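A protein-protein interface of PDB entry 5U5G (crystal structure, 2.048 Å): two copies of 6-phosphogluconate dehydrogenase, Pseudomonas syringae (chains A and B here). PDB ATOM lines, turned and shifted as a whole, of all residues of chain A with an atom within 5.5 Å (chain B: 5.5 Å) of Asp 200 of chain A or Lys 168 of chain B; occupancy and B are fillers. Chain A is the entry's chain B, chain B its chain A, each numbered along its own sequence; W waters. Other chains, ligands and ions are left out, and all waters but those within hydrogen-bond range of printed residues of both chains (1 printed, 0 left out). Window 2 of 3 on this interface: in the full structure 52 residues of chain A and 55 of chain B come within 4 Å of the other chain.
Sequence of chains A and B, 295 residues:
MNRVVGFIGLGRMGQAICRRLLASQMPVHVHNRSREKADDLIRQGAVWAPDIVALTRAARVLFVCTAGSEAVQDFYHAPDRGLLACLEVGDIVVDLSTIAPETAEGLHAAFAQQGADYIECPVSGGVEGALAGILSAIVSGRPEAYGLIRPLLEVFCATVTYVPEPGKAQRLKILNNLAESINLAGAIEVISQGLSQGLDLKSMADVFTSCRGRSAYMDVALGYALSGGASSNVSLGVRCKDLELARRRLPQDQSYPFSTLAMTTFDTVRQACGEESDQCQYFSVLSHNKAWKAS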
ATOM      1  N   LEU A 195      16.162   4.845  -6.529  1.00  0.00           N
ATOM      2  CA  LEU A 195      15.212   3.744  -6.649  1.00  0.00           C
ATOM      3  C   LEU A 195      13.949   4.196  -7.372  1.00  0.00           C
ATOM      4  O   LEU A 195      13.481   3.525  -8.299  1.00  0.00           O
ATOM      5  CB  LEU A 195      14.882   3.169  -5.265  1.00  0.00           C
ATOM      6  CG  LEU A 195      16.025   2.417  -4.569  1.00  0.00           C
ATOM      7  CD1 LEU A 195      15.656   1.989  -3.144  1.00  0.00           C
ATOM      8  CD2 LEU A 195      16.500   1.204  -5.386  1.00  0.00           C
ATOM      9  N   GLY A 198      14.232   4.280 -10.997  1.00  0.00           N
ATOM     10  CA  GLY A 198      14.482   3.021 -11.667  1.00  0.00           C
ATOM     11  C   GLY A 198      15.929   2.601 -11.759  1.00  0.00           C
ATOM     12  O   GLY A 198      16.251   1.740 -12.579  1.00  0.00           O
ATOM     13  N   LEU A 199      16.820   3.178 -10.957  1.00  0.00           N
ATOM     14  CA  LEU A 199      18.195   2.696 -10.903  1.00  0.00           C
ATOM     15  C   LEU A 199      18.278   1.480  -9.991  1.00  0.00           C
ATOM     16  O   LEU A 199      17.630   1.427  -8.938  1.00  0.00           O
ATOM     17  CB  LEU A 199      19.140   3.789 -10.393  1.00  0.00           C
ATOM     18  CG  LEU A 199      19.184   5.087 -11.198  1.00  0.00           C
ATOM     19  CD1 LEU A 199      20.029   6.141 -10.488  1.00  0.00           C
ATOM     20  CD2 LEU A 199      19.698   4.829 -12.611  1.00  0.00           C
ATOM     21  N   ASP A 200      19.081   0.503 -10.388  1.00  0.00           N
ATOM     22  CA  ASP A 200      19.308  -0.642  -9.520  1.00  0.00           C
ATOM     23  C   ASP A 200      20.270  -0.274  -8.399  1.00  0.00           C
ATOM     24  O   ASP A 200      21.127   0.608  -8.547  1.00  0.00           O
ATOM     25  CB  ASP A 200      19.875  -1.816 -10.312  1.00  0.00           C
ATOM     26  CG  ASP A 200      21.125  -1.446 -11.061  1.00  0.00           C
ATOM     27  OD1 ASP A 200      21.056  -0.514 -11.887  1.00  0.00           O
ATOM     28  OD2 ASP A 200      22.176  -2.062 -10.790  1.00  0.00           O
ATOM     29  N   LEU A 201      20.121  -0.971  -7.266  1.00  0.00           N
ATOM     30  CA  LEU A 201      20.985  -0.741  -6.114  1.00  0.00           C
ATOM     31  C   LEU A 201      22.441  -1.043  -6.437  1.00  0.00           C
ATOM     32  O   LEU A 201      23.345  -0.325  -5.992  1.00  0.00           O
ATOM     33  CB  LEU A 201      20.544  -1.608  -4.936  1.00  0.00           C
ATOM     34  CG  LEU A 201      19.632  -1.021  -3.872  1.00  0.00           C
ATOM     35  CD1 LEU A 201      19.419  -2.065  -2.786  1.00  0.00           C
ATOM     36  CD2 LEU A 201      20.254   0.224  -3.301  1.00  0.00           C
ATOM     37  N   LYS A 202      22.684  -2.123  -7.186  1.00  0.00           N
ATOM     38  CA  LYS A 202      24.046  -2.493  -7.556  1.00  0.00           C
ATOM     39  C   LYS A 202      24.757  -1.353  -8.273  1.00  0.00           C
ATOM     40  O   LYS A 202      25.905  -1.036  -7.952  1.00  0.00           O
ATOM     41  CB  LYS A 202      24.028  -3.751  -8.428  1.00  0.00           C
ATOM     42  CG  LYS A 202      25.238  -3.880  -9.332  1.00  0.00           C
ATOM     43  CD  LYS A 202      25.975  -5.172  -9.114  1.00  0.00           C
ATOM     44  CE  LYS A 202      27.148  -5.275 -10.075  1.00  0.00           C
ATOM     45  NZ  LYS A 202      28.230  -4.329  -9.687  1.00  0.00           N
ATOM     46  N   SER A 203      24.088  -0.715  -9.245  1.00  0.00           N
ATOM     47  CA  SER A 203      24.713   0.403  -9.956  1.00  0.00           C
ATOM     48  C   SER A 203      25.013   1.558  -9.014  1.00  0.00           C
ATOM     49  O   SER A 203      26.105   2.141  -9.047  1.00  0.00           O
ATOM     50  CB  SER A 203      23.811   0.892 -11.084  1.00  0.00           C
ATOM     51  OG  SER A 203      23.853  -0.045 -12.141  1.00  0.00           O
ATOM     52  N   MET A 204      24.035   1.927  -8.190  1.00  0.00           N
ATOM     53  CA  MET A 204      24.242   3.019  -7.251  1.00  0.00           C
ATOM     54  C   MET A 204      25.370   2.690  -6.285  1.00  0.00           C
ATOM     55  O   MET A 204      26.184   3.556  -5.952  1.00  0.00           O
ATOM     56  CB  MET A 204      22.939   3.316  -6.514  1.00  0.00           C
ATOM     57  CG  MET A 204      21.872   3.958  -7.384  1.00  0.00           C
ATOM     58  SD  MET A 204      20.476   4.563  -6.410  1.00  0.00           S
ATOM     59  CE  MET A 204      19.526   3.040  -6.265  1.00  0.00           C
ATOM     60  N   ALA A 205      25.459   1.432  -5.854  1.00  0.00           N
ATOM     61  CA  ALA A 205      26.544   1.051  -4.953  1.00  0.00           C
ATOM     62  C   ALA A 205      27.904   1.162  -5.637  1.00  0.00           C
ATOM     63  O   ALA A 205      28.878   1.607  -5.021  1.00  0.00           O
ATOM     64  CB  ALA A 205      26.323  -0.369  -4.424  1.00  0.00           C
ATOM     65  N   GLU B 105      20.499  10.874 -24.033  1.00  0.00           N
ATOM     66  CA  GLU B 105      19.721   9.915 -24.813  1.00  0.00           C
ATOM     67  C   GLU B 105      19.535  10.394 -26.247  1.00  0.00           C
ATOM     68  O   GLU B 105      19.711   9.622 -27.197  1.00  0.00           O
ATOM     69  CB  GLU B 105      18.373   9.677 -24.144  1.00  0.00           C
ATOM     70  CG  GLU B 105      18.475   8.766 -22.933  1.00  0.00           C
ATOM     71  CD  GLU B 105      17.254   8.829 -22.035  1.00  0.00           C
ATOM     72  OE1 GLU B 105      16.327   9.609 -22.342  1.00  0.00           O
ATOM     73  OE2 GLU B 105      17.236   8.110 -21.011  1.00  0.00           O
ATOM     74  N   GLU B 120      28.662   8.077 -23.464  1.00  0.00           N
ATOM     75  CA  GLU B 120      28.258   8.944 -22.365  1.00  0.00           C
ATOM     76  C   GLU B 120      29.129   8.596 -21.159  1.00  0.00           C
ATOM     77  O   GLU B 120      28.989   7.516 -20.586  1.00  0.00           O
ATOM     78  CB  GLU B 120      26.765   8.726 -22.111  1.00  0.00           C
ATOM     79  CG  GLU B 120      26.151   9.267 -20.838  1.00  0.00           C
ATOM     80  CD  GLU B 120      24.720   8.739 -20.628  1.00  0.00           C
ATOM     81  OE1 GLU B 120      24.094   8.252 -21.600  1.00  0.00           O
ATOM     82  OE2 GLU B 120      24.229   8.791 -19.486  1.00  0.00           O
ATOM     83  N   ILE B 138      31.581   6.743 -15.191  1.00  0.00           N
ATOM     84  CA  ILE B 138      30.313   6.037 -15.364  1.00  0.00           C
ATOM     85  C   ILE B 138      29.974   6.104 -16.846  1.00  0.00           C
ATOM     86  O   ILE B 138      29.976   7.190 -17.430  1.00  0.00           O
ATOM     87  CB  ILE B 138      29.184   6.666 -14.527  1.00  0.00           C
ATOM     88  CG1 ILE B 138      29.717   7.126 -13.167  1.00  0.00           C
ATOM     89  CG2 ILE B 138      27.997   5.697 -14.417  1.00  0.00           C
ATOM     90  CD1 ILE B 138      28.869   8.215 -12.518  1.00  0.00           C
ATOM     91  N   SER B 140      27.771   4.929 -20.341  1.00  0.00           N
ATOM     92  CA  SER B 140      26.640   4.378 -21.070  1.00  0.00           C
ATOM     93  C   SER B 140      26.927   4.424 -22.566  1.00  0.00           C
ATOM     94  O   SER B 140      27.620   5.323 -23.057  1.00  0.00           O
ATOM     95  CB  SER B 140      25.346   5.147 -20.790  1.00  0.00           C
ATOM     96  OG  SER B 140      24.949   5.032 -19.444  1.00  0.00           O
ATOM     97  N   VAL B 163      27.381   1.040 -17.485  1.00  0.00           N
ATOM     98  CA  VAL B 163      25.935   0.875 -17.363  1.00  0.00           C
ATOM     99  C   VAL B 163      25.319   1.204 -18.725  1.00  0.00           C
ATOM    100  O   VAL B 163      24.971   2.364 -18.999  1.00  0.00           O
ATOM    101  CB  VAL B 163      25.373   1.734 -16.216  1.00  0.00           C
ATOM    102  CG1 VAL B 163      25.651   1.060 -14.865  1.00  0.00           C
ATOM    103  CG2 VAL B 163      25.993   3.163 -16.234  1.00  0.00           C
ATOM    104  N   GLU B 165      22.689   1.282 -20.691  1.00  0.00           N
ATOM    105  CA  GLU B 165      21.475   1.987 -21.091  1.00  0.00           C
ATOM    106  C   GLU B 165      21.731   3.483 -21.254  1.00  0.00           C
ATOM    107  O   GLU B 165      22.226   4.127 -20.319  1.00  0.00           O
ATOM    108  CB  GLU B 165      20.377   1.764 -20.055  1.00  0.00           C
ATOM    109  CG  GLU B 165      19.097   2.536 -20.333  1.00  0.00           C
ATOM    110  CD  GLU B 165      18.070   2.416 -19.204  1.00  0.00           C
ATOM    111  OE1 GLU B 165      18.477   2.259 -18.032  1.00  0.00           O
ATOM    112  OE2 GLU B 165      16.853   2.467 -19.492  1.00  0.00           O
ATOM    113  N   PRO B 166      21.394   4.069 -22.407  1.00  0.00           N
ATOM    114  CA  PRO B 166      21.600   5.512 -22.600  1.00  0.00           C
ATOM    115  C   PRO B 166      20.923   6.341 -21.519  1.00  0.00           C
ATOM    116  O   PRO B 166      19.791   6.070 -21.108  1.00  0.00           O
ATOM    117  CB  PRO B 166      20.974   5.778 -23.973  1.00  0.00           C
ATOM    118  CG  PRO B 166      21.073   4.459 -24.697  1.00  0.00           C
ATOM    119  CD  PRO B 166      20.897   3.402 -23.624  1.00  0.00           C
ATOM    120  N   GLY B 167      21.626   7.375 -21.064  1.00  0.00           N
ATOM    121  CA  GLY B 167      21.116   8.239 -20.029  1.00  0.00           C
ATOM    122  C   GLY B 167      21.359   7.750 -18.620  1.00  0.00           C
ATOM    123  O   GLY B 167      21.241   8.544 -17.681  1.00  0.00           O
ATOM    124  N   LYS B 168      21.717   6.472 -18.444  1.00  0.00           N
ATOM    125  CA  LYS B 168      21.857   5.922 -17.096  1.00  0.00           C
ATOM    126  C   LYS B 168      23.089   6.479 -16.394  1.00  0.00           C
ATOM    127  O   LYS B 168      23.049   6.752 -15.189  1.00  0.00           O
ATOM    128  CB  LYS B 168      21.916   4.395 -17.137  1.00  0.00           C
ATOM    129  CG  LYS B 168      21.996   3.757 -15.745  1.00  0.00           C
ATOM    130  CD  LYS B 168      21.687   2.251 -15.775  1.00  0.00           C
ATOM    131  CE  LYS B 168      21.670   1.685 -14.373  1.00  0.00           C
ATOM    132  NZ  LYS B 168      21.381   0.236 -14.347  1.00  0.00           N
ATOM    133  N   ALA B 169      24.197   6.637 -17.124  1.00  0.00           N
ATOM    134  CA  ALA B 169      25.392   7.210 -16.516  1.00  0.00           C
ATOM    135  C   ALA B 169      25.118   8.612 -15.991  1.00  0.00           C
ATOM    136  O   ALA B 169      25.553   8.962 -14.887  1.00  0.00           O
ATOM    137  CB  ALA B 169      26.549   7.222 -17.520  1.00  0.00           C
ATOM    138  N   GLN B 170      24.387   9.432 -16.757  1.00  0.00           N
ATOM    139  CA  GLN B 170      24.109  10.783 -16.275  1.00  0.00           C
ATOM    140  C   GLN B 170      23.177  10.751 -15.075  1.00  0.00           C
ATOM    141  O   GLN B 170      23.327  11.558 -14.154  1.00  0.00           O
ATOM    142  CB  GLN B 170      23.516  11.663 -17.378  1.00  0.00           C
ATOM    143  CG  GLN B 170      24.486  12.007 -18.522  1.00  0.00           C
ATOM    144  CD  GLN B 170      25.678  12.848 -18.072  1.00  0.00           C
ATOM    145  OE1 GLN B 170      25.689  13.420 -16.978  1.00  0.00           O
ATOM    146  NE2 GLN B 170      26.678  12.934 -18.921  1.00  0.00           N
ATOM    147  N   ARG B 171      22.207   9.834 -15.071  1.00  0.00           N
ATOM    148  CA  ARG B 171      21.325   9.702 -13.914  1.00  0.00           C
ATOM    149  C   ARG B 171      22.133   9.448 -12.651  1.00  0.00           C
ATOM    150  O   ARG B 171      21.917  10.098 -11.622  1.00  0.00           O
ATOM    151  CB  ARG B 171      20.315   8.574 -14.144  1.00  0.00           C
ATOM    152  CG  ARG B 171      19.296   8.901 -15.221  1.00  0.00           C
ATOM    153  CD  ARG B 171      18.324   7.756 -15.526  1.00  0.00           C
ATOM    154  NE  ARG B 171      17.403   8.206 -16.569  1.00  0.00           N
ATOM    155  CZ  ARG B 171      17.449   7.835 -17.848  1.00  0.00           C
ATOM    156  NH1 ARG B 171      18.339   6.945 -18.273  1.00  0.00           N
ATOM    157  NH2 ARG B 171      16.575   8.338 -18.702  1.00  0.00           N
ATOM    158  N   LEU B 172      23.087   8.515 -12.725  1.00  0.00           N
ATOM    159  CA  LEU B 172      23.911   8.167 -11.571  1.00  0.00           C
ATOM    160  C   LEU B 172      24.847   9.309 -11.171  1.00  0.00           C
ATOM    161  O   LEU B 172      25.051   9.570  -9.975  1.00  0.00           O
ATOM    162  CB  LEU B 172      24.702   6.902 -11.890  1.00  0.00           C
ATOM    163  CG  LEU B 172      23.817   5.653 -11.951  1.00  0.00           C
ATOM    164  CD1 LEU B 172      24.507   4.556 -12.742  1.00  0.00           C
ATOM    165  CD2 LEU B 172      23.499   5.199 -10.530  1.00  0.00           C
ATOM    166  N   LYS B 173      25.441   9.982 -12.156  1.00  0.00           N
ATOM    167  CA  LYS B 173      26.353  11.082 -11.866  1.00  0.00           C
ATOM    168  C   LYS B 173      25.639  12.211 -11.133  1.00  0.00           C
ATOM    169  O   LYS B 173      26.159  12.740 -10.143  1.00  0.00           O
ATOM    170  CB  LYS B 173      26.982  11.598 -13.174  1.00  0.00           C
ATOM    171  CG  LYS B 173      27.708  12.966 -13.057  1.00  0.00           C
ATOM    172  CD  LYS B 173      29.029  12.849 -12.261  1.00  0.00           C
ATOM    173  CE  LYS B 173      29.744  14.233 -12.155  1.00  0.00           C
ATOM    174  NZ  LYS B 173      30.839  14.223 -11.127  1.00  0.00           N
HETATM  175  O   HOH W   1      18.385   0.744 -13.997  1.00  0.00           O
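Of the printed residues of chain B, Leu 199 of chain A touches Leu 172. Of chain B, only Lys 168 comes within 4 Å of Asp 200 of chain A. Of the printed residues of chain A, Val 163 of chain B touches Ser 203 (3.4 Å). Of chain A, only Asp 200 and Ser 203 come within 4 Å of Lys 168 of chain B. Of the printed residues of chain A, Leu 172 of chain B touches Leu 199 (3.6 Å) and Met 204 (3.8 Å). The nearest residue of chain A that does not touch Lys 168 of chain B is Leu 199 of chain A (4.03 Å).
The side-chain hydroxyl (OG) of Ser 140 of chain B is in hydrogen-bond range of the backbone carbonyl oxygen (O) of Val 163 of chain B, at 2.7 Å. The side-chain carboxylate of Asp 200 of chain A sits at hydrogen-bond distance from the backbone NH of Ser 203 of chain A, 2.8 Å away.
Of the 14 printed residues of chain B, 3 touch a printed residue of chain A. Printed residues of chain B that touch a printed residue of chain A: Val 163, Lys 168 and Leu 172.
No position is printed for both chains. Of the 5 pairs that touch across the chains among the printed residues, none has its exchanged pair printed and touching as well.
Water W1 lies within hydrogen-bond range of the backbone carbonyl oxygen (O) of Gly 198 of chain A and the side-chain amino group (NZ) of Lys 168 of chain B.
The side-chain amino group (NZ) of Lys 168 of chain B is in salt-bridge range of the side-chain carboxylate (OD1) of Asp 200 of chain A. The side-chain amino group (NZ) of Lys 168 of chain B sits at hydrogen-bond distance from the side-chain hydroxyl (OG) of Ser 203 of chain A.
CD2 of Leu 172 of chain B touches CD1 of Leu 199 of chain A, 3.6 Å away. Ser 203 of chain A touches Val 163 of chain B. CD2 of Leu 172 of chain B touches CG of Met 204 of chain A, at 3.8 Å.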
